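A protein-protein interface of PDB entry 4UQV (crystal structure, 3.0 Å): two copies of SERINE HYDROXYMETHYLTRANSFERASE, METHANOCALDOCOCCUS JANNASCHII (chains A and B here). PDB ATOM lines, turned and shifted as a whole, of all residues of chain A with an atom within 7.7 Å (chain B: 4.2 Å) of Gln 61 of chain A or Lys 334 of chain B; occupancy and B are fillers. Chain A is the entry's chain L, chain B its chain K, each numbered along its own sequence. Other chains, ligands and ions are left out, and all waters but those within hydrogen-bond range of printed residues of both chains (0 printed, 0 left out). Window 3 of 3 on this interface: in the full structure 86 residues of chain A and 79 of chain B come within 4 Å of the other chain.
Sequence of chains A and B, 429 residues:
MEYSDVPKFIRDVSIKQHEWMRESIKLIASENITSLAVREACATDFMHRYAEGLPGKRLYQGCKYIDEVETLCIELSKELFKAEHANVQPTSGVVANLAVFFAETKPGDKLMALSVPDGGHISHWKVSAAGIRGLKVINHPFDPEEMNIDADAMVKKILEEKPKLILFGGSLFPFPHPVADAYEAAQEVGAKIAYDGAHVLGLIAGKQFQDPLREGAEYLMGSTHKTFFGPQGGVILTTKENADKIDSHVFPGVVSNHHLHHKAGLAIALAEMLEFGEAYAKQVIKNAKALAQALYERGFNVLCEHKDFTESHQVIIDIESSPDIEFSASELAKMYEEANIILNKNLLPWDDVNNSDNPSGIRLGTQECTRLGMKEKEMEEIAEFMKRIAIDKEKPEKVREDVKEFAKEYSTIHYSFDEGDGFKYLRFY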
ATOM      1  N   ARG A  49      28.769   4.887  -6.362  1.00  0.00           N
ATOM      2  CA  ARG A  49      27.944   5.616  -5.401  1.00  0.00           C
ATOM      3  C   ARG A  49      26.442   5.316  -5.428  1.00  0.00           C
ATOM      4  O   ARG A  49      25.948   4.588  -6.290  1.00  0.00           O
ATOM      5  CB  ARG A  49      28.138   7.114  -5.615  1.00  0.00           C
ATOM      6  CG  ARG A  49      28.532   7.871  -4.371  1.00  0.00           C
ATOM      7  CD  ARG A  49      28.849   9.308  -4.711  1.00  0.00           C
ATOM      8  NE  ARG A  49      29.491   9.990  -3.597  1.00  0.00           N
ATOM      9  CZ  ARG A  49      30.003  11.212  -3.669  1.00  0.00           C
ATOM     10  NH1 ARG A  49      29.951  11.892  -4.801  1.00  0.00           N
ATOM     11  NH2 ARG A  49      30.571  11.756  -2.604  1.00  0.00           N
ATOM     12  N   TYR A  50      25.733   5.903  -4.465  1.00  0.00           N
ATOM     13  CA  TYR A  50      24.278   5.807  -4.360  1.00  0.00           C
ATOM     14  C   TYR A  50      23.664   7.102  -3.824  1.00  0.00           C
ATOM     15  O   TYR A  50      24.126   7.647  -2.824  1.00  0.00           O
ATOM     16  CB  TYR A  50      23.879   4.630  -3.465  1.00  0.00           C
ATOM     17  CG  TYR A  50      23.852   3.307  -4.192  1.00  0.00           C
ATOM     18  CD1 TYR A  50      22.722   2.904  -4.891  1.00  0.00           C
ATOM     19  CD2 TYR A  50      24.957   2.466  -4.186  1.00  0.00           C
ATOM     20  CE1 TYR A  50      22.691   1.700  -5.564  1.00  0.00           C
ATOM     21  CE2 TYR A  50      24.935   1.259  -4.855  1.00  0.00           C
ATOM     22  CZ  TYR A  50      23.799   0.881  -5.543  1.00  0.00           C
ATOM     23  OH  TYR A  50      23.770  -0.317  -6.214  1.00  0.00           O
ATOM     24  N   ARG A  58      19.222  11.313   1.157  1.00  0.00           N
ATOM     25  CA  ARG A  58      19.790   9.968   1.169  1.00  0.00           C
ATOM     26  C   ARG A  58      19.675   9.277   2.523  1.00  0.00           C
ATOM     27  O   ARG A  58      19.750   9.918   3.572  1.00  0.00           O
ATOM     28  CB  ARG A  58      21.261  10.000   0.751  1.00  0.00           C
ATOM     29  CG  ARG A  58      21.611   9.095  -0.429  1.00  0.00           C
ATOM     30  CD  ARG A  58      21.268   7.622  -0.194  1.00  0.00           C
ATOM     31  NE  ARG A  58      21.096   6.913  -1.462  1.00  0.00           N
ATOM     32  CZ  ARG A  58      20.496   5.733  -1.598  1.00  0.00           C
ATOM     33  NH1 ARG A  58      20.000   5.107  -0.540  1.00  0.00           N
ATOM     34  NH2 ARG A  58      20.389   5.179  -2.800  1.00  0.00           N
ATOM     35  N   LEU A  59      19.494   7.961   2.479  1.00  0.00           N
ATOM     36  CA  LEU A  59      19.555   7.125   3.669  1.00  0.00           C
ATOM     37  C   LEU A  59      20.986   6.630   3.860  1.00  0.00           C
ATOM     38  O   LEU A  59      21.287   5.876   4.786  1.00  0.00           O
ATOM     39  CB  LEU A  59      18.575   5.956   3.560  1.00  0.00           C
ATOM     40  CG  LEU A  59      17.109   6.376   3.412  1.00  0.00           C
ATOM     41  CD1 LEU A  59      16.177   5.178   3.526  1.00  0.00           C
ATOM     42  CD2 LEU A  59      16.741   7.446   4.435  1.00  0.00           C
ATOM     43  N   TYR A  60      21.859   7.062   2.956  1.00  0.00           N
ATOM     44  CA  TYR A  60      23.299   6.897   3.101  1.00  0.00           C
ATOM     45  C   TYR A  60      23.907   8.287   3.249  1.00  0.00           C
ATOM     46  O   TYR A  60      23.185   9.282   3.278  1.00  0.00           O
ATOM     47  CB  TYR A  60      23.912   6.173   1.898  1.00  0.00           C
ATOM     48  CG  TYR A  60      23.254   4.858   1.529  1.00  0.00           C
ATOM     49  CD1 TYR A  60      22.649   4.058   2.493  1.00  0.00           C
ATOM     50  CD2 TYR A  60      23.242   4.416   0.211  1.00  0.00           C
ATOM     51  CE1 TYR A  60      22.047   2.856   2.151  1.00  0.00           C
ATOM     52  CE2 TYR A  60      22.645   3.219  -0.139  1.00  0.00           C
ATOM     53  CZ  TYR A  60      22.049   2.443   0.833  1.00  0.00           C
ATOM     54  OH  TYR A  60      21.455   1.250   0.484  1.00  0.00           O
ATOM     55  N   GLN A  61      25.229   8.361   3.340  1.00  0.00           N
ATOM     56  CA  GLN A  61      25.904   9.652   3.384  1.00  0.00           C
ATOM     57  C   GLN A  61      27.078   9.675   2.412  1.00  0.00           C
ATOM     58  O   GLN A  61      27.368   8.678   1.749  1.00  0.00           O
ATOM     59  CB  GLN A  61      26.378   9.968   4.804  1.00  0.00           C
ATOM     60  CG  GLN A  61      25.251  10.145   5.815  1.00  0.00           C
ATOM     61  CD  GLN A  61      24.938  11.600   6.107  1.00  0.00           C
ATOM     62  OE1 GLN A  61      23.792  11.960   6.378  1.00  0.00           O
ATOM     63  NE2 GLN A  61      25.960  12.443   6.067  1.00  0.00           N
ATOM     64  N   GLY A  62      27.752  10.817   2.335  1.00  0.00           N
ATOM     65  CA  GLY A  62      28.874  10.982   1.430  1.00  0.00           C
ATOM     66  C   GLY A  62      28.446  11.362   0.028  1.00  0.00           C
ATOM     67  O   GLY A  62      29.226  11.267  -0.912  1.00  0.00           O
ATOM     68  N   CYS A  63      27.194  11.781  -0.107  1.00  0.00           N
ATOM     69  CA  CYS A  63      26.650  12.245  -1.377  1.00  0.00           C
ATOM     70  C   CYS A  63      26.736  13.765  -1.509  1.00  0.00           C
ATOM     71  O   CYS A  63      26.145  14.341  -2.419  1.00  0.00           O
ATOM     72  CB  CYS A  63      25.206  11.775  -1.545  1.00  0.00           C
ATOM     73  SG  CYS A  63      24.309  11.551   0.007  1.00  0.00           S
ATOM     74  N   LYS A  64      27.449  14.406  -0.584  1.00  0.00           N
ATOM     75  CA  LYS A  64      27.467  15.866  -0.452  1.00  0.00           C
ATOM     76  C   LYS A  64      27.610  16.623  -1.774  1.00  0.00           C
ATOM     77  O   LYS A  64      26.967  17.655  -1.969  1.00  0.00           O
ATOM     78  CB  LYS A  64      28.599  16.286   0.491  1.00  0.00           C
ATOM     79  CG  LYS A  64      28.461  17.701   1.035  1.00  0.00           C
ATOM     80  CD  LYS A  64      29.664  18.095   1.876  1.00  0.00           C
ATOM     81  CE  LYS A  64      30.823  18.536   1.003  1.00  0.00           C
ATOM     82  NZ  LYS A  64      30.481  19.753   0.215  1.00  0.00           N
ATOM     83  N   SER B 330      22.665   9.377  12.810  1.00  0.00           N
ATOM     84  CA  SER B 330      22.958  10.389  11.803  1.00  0.00           C
ATOM     85  C   SER B 330      23.823  11.492  12.400  1.00  0.00           C
ATOM     86  O   SER B 330      24.602  12.137  11.692  1.00  0.00           O
ATOM     87  CB  SER B 330      21.667  10.975  11.229  1.00  0.00           C
ATOM     88  OG  SER B 330      21.913  11.678  10.025  1.00  0.00           O
ATOM     89  N   LEU B 332      26.326  11.100  14.295  1.00  0.00           N
ATOM     90  CA  LEU B 332      27.691  10.684  14.004  1.00  0.00           C
ATOM     91  C   LEU B 332      27.946  10.715  12.503  1.00  0.00           C
ATOM     92  O   LEU B 332      28.984  11.196  12.052  1.00  0.00           O
ATOM     93  CB  LEU B 332      27.967   9.279  14.546  1.00  0.00           C
ATOM     94  CG  LEU B 332      27.793   9.025  16.043  1.00  0.00           C
ATOM     95  CD1 LEU B 332      28.518   7.752  16.432  1.00  0.00           C
ATOM     96  CD2 LEU B 332      28.296  10.198  16.860  1.00  0.00           C
ATOM     97  N   ALA B 333      26.982  10.200  11.743  1.00  0.00           N
ATOM     98  CA  ALA B 333      27.134   9.999  10.304  1.00  0.00           C
ATOM     99  C   ALA B 333      27.527  11.266   9.546  1.00  0.00           C
ATOM    100  O   ALA B 333      28.383  11.222   8.664  1.00  0.00           O
ATOM    101  CB  ALA B 333      25.850   9.424   9.724  1.00  0.00           C
ATOM    102  N   LYS B 334      26.903  12.390   9.889  1.00  0.00           N
ATOM    103  CA  LYS B 334      27.181  13.651   9.203  1.00  0.00           C
ATOM    104  C   LYS B 334      28.606  14.141   9.452  1.00  0.00           C
ATOM    105  O   LYS B 334      29.386  14.349   8.512  1.00  0.00           O
ATOM    106  CB  LYS B 334      26.182  14.721   9.646  1.00  0.00           C
ATOM    107  CG  LYS B 334      24.739  14.382   9.321  1.00  0.00           C
ATOM    108  CD  LYS B 334      23.789  14.974  10.348  1.00  0.00           C
ATOM    109  CE  LYS B 334      22.346  14.812   9.907  1.00  0.00           C
ATOM    110  NZ  LYS B 334      21.390  15.317  10.926  1.00  0.00           N
ATOM    111  N   MET B 335      28.941  14.306  10.729  1.00  0.00           N
ATOM    112  CA  MET B 335      30.266  14.761  11.128  1.00  0.00           C
ATOM    113  C   MET B 335      31.331  13.835  10.559  1.00  0.00           C
ATOM    114  O   MET B 335      32.423  14.274  10.200  1.00  0.00           O
ATOM    115  CB  MET B 335      30.371  14.831  12.651  1.00  0.00           C
ATOM    116  CG  MET B 335      29.251  15.621  13.304  1.00  0.00           C
ATOM    117  SD  MET B 335      29.446  15.757  15.087  1.00  0.00           S
ATOM    118  CE  MET B 335      29.493  14.031  15.568  1.00  0.00           C
ATOM    119  N   TYR B 336      30.995  12.552  10.474  1.00  0.00           N
ATOM    120  CA  TYR B 336      31.841  11.574   9.808  1.00  0.00           C
ATOM    121  C   TYR B 336      32.003  11.932   8.335  1.00  0.00           C
ATOM    122  O   TYR B 336      33.111  11.897   7.802  1.00  0.00           O
ATOM    123  CB  TYR B 336      31.256  10.166   9.954  1.00  0.00           C
ATOM    124  CG  TYR B 336      31.533   9.516  11.291  1.00  0.00           C
ATOM    125  CD1 TYR B 336      32.622   9.905  12.059  1.00  0.00           C
ATOM    126  CD2 TYR B 336      30.711   8.510  11.784  1.00  0.00           C
ATOM    127  CE1 TYR B 336      32.885   9.315  13.283  1.00  0.00           C
ATOM    128  CE2 TYR B 336      30.965   7.912  13.006  1.00  0.00           C
ATOM    129  CZ  TYR B 336      32.053   8.319  13.752  1.00  0.00           C
ATOM    130  OH  TYR B 336      32.311   7.731  14.970  1.00  0.00           O
ATOM    131  N   GLU B 337      30.895  12.286   7.687  1.00  0.00           N
ATOM    132  CA  GLU B 337      30.915  12.620   6.266  1.00  0.00           C
ATOM    133  C   GLU B 337      31.831  13.808   5.994  1.00  0.00           C
ATOM    134  O   GLU B 337      32.519  13.843   4.974  1.00  0.00           O
ATOM    135  CB  GLU B 337      29.501  12.915   5.748  1.00  0.00           C
ATOM    136  CG  GLU B 337      29.450  13.259   4.261  1.00  0.00           C
ATOM    137  CD  GLU B 337      28.058  13.639   3.780  1.00  0.00           C
ATOM    138  OE1 GLU B 337      27.132  13.705   4.615  1.00  0.00           O
ATOM    139  OE2 GLU B 337      27.891  13.873   2.564  1.00  0.00           O
ATOM    140  N   GLU B 338      31.852  14.777   6.906  1.00  0.00           N
ATOM    141  CA  GLU B 338      32.770  15.906   6.744  1.00  0.00           C
ATOM    142  C   GLU B 338      34.121  15.652   7.414  1.00  0.00           C
ATOM    143  O   GLU B 338      34.986  16.527   7.431  1.00  0.00           O
ATOM    144  CB  GLU B 338      32.155  17.202   7.283  1.00  0.00           C
ATOM    145  CG  GLU B 338      31.378  17.054   8.574  1.00  0.00           C
ATOM    146  CD  GLU B 338      29.880  17.179   8.363  1.00  0.00           C
ATOM    147  OE1 GLU B 338      29.426  17.036   7.208  1.00  0.00           O
ATOM    148  OE2 GLU B 338      29.155  17.413   9.355  1.00  0.00           O
ATOM    149  N   ILE B 342      33.208   8.075   5.556  1.00  0.00           N
ATOM    150  CA  ILE B 342      31.799   8.086   5.167  1.00  0.00           C
ATOM    151  C   ILE B 342      31.150   6.716   5.308  1.00  0.00           C
ATOM    152  O   ILE B 342      31.664   5.736   4.772  1.00  0.00           O
ATOM    153  CB  ILE B 342      31.630   8.556   3.706  1.00  0.00           C
ATOM    154  CG1 ILE B 342      32.005  10.036   3.555  1.00  0.00           C
ATOM    155  CG2 ILE B 342      30.214   8.304   3.235  1.00  0.00           C
ATOM    156  CD1 ILE B 342      33.487  10.288   3.293  1.00  0.00           C
ATOM    157  N   ASN B 344      26.951   5.672   6.515  1.00  0.00           N
ATOM    158  CA  ASN B 344      25.513   5.650   6.192  1.00  0.00           C
ATOM    159  C   ASN B 344      24.625   6.197   7.311  1.00  0.00           C
ATOM    160  O   ASN B 344      25.116   6.712   8.315  1.00  0.00           O
ATOM    161  CB  ASN B 344      25.093   4.301   5.602  1.00  0.00           C
ATOM    162  CG  ASN B 344      25.596   3.130   6.413  1.00  0.00           C
ATOM    163  OD1 ASN B 344      25.827   3.247   7.614  1.00  0.00           O
ATOM    164  ND2 ASN B 344      25.774   1.986   5.755  1.00  0.00           N
ATOM    165  N   LYS B 345      23.313   6.066   7.131  1.00  0.00           N
ATOM    166  CA  LYS B 345      22.305   6.100   8.187  1.00  0.00           C
ATOM    167  C   LYS B 345      21.426   4.854   8.087  1.00  0.00           C
ATOM    168  O   LYS B 345      20.610   4.743   7.171  1.00  0.00           O
ATOM    169  CB  LYS B 345      21.448   7.360   8.075  1.00  0.00           C
ATOM    170  CG  LYS B 345      22.241   8.645   7.929  1.00  0.00           C
ATOM    171  CD  LYS B 345      21.545   9.600   6.973  1.00  0.00           C
ATOM    172  CE  LYS B 345      20.094   9.814   7.364  1.00  0.00           C
ATOM    173  NZ  LYS B 345      19.367  10.655   6.373  1.00  0.00           N
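The backbone NH (N) of Lys 345 of chain B is in hydrogen-bond range of the backbone carbonyl oxygen (O) of Leu 59 of chain A (3.1 Å). OE1 of Glu 337 of chain B lies close to NE2 of Gln 61 of chain A (2.3 Å). The side-chain carboxylate (OE2) of Glu 337 of chain B sits at hydrogen-bond distance from the backbone NH (N) of Gly 62 of chain A (3.1 Å). N of Lys 64 of chain A lies within hydrogen-bond range of OE2 of Glu 337 of chain B (3.2 Å). NZ of Lys 345 of chain B sits at hydrogen-bond distance from O of Arg 58 of chain A (2.9 Å). N of Cys 63 of chain A sits at hydrogen-bond distance from OE2 of Glu 337 of chain B (3.5 Å).
NE of Arg 49 of chain A lies close to O of Gly 62 of chain A, 3.0 Å away. NE of Arg 58 of chain A sits at hydrogen-bond distance from O of Tyr 50 of chain A (3.4 Å).
Among the printed residues, pairs that only touch across the chains: Tyr 60 of chain A with Asn 344 of chain B, Gln 61 of chain A with Ala 333 of chain B, Gln 61 of chain A with Lys 334 of chain B, Gln 61 of chain A with Ile 342 of chain B, Gln 61 of chain A with Asn 344 of chain B, Gln 61 of chain A with Lys 345 of chain B and Gly 62 of chain A with Ile 342 of chain B.
Tyr 50 of chain A touches none of the printed residues of chain B. Of the printed residues of chain B, Leu 59 of chain A touches Lys 345 (2.7 Å). Printed residues of chain B within 4 Å of Gln 61 of chain A: Ala 333, Lys 334, Glu 337, Ile 342, Asn 344 and Lys 345. Of the printed residues of chain B, Cys 63 of chain A touches Glu 337. Leu 332 of chain B touches none of the printed residues of chain A. Of chain A, only Gln 61 (3.8 Å) comes within 4 Å of Ala 333 of chain B. Lys 334 of chain B touches one residue of chain A. Of the printed residues of chain A, Ile 342 of chain B touches Gln 61 (3.2 Å) and Gly 62 (3.5 Å). Printed residues of chain A within 4 Å of Asn 344 of chain B: Tyr 60 and Gln 61. The nearest residue of chain A that does not touch Lys 334 of chain B is Gly 62 of chain A (7.3 Å).
Of the 9 printed residues of chain A, 7 touch a printed residue of chain B. Of the 11 printed residues of chain B, 6 touch a printed residue of chain A. Hydrophobic or aromatic side chains of chain B within 4 Å of the printed part of chain A: Ile 342. Among the printed residues, 13 pairs touch across the chains.
No position is printed for both chains. Of the 13 pairs that touch across the chains among the printed residues, none has its exchanged pair printed and touching as well.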
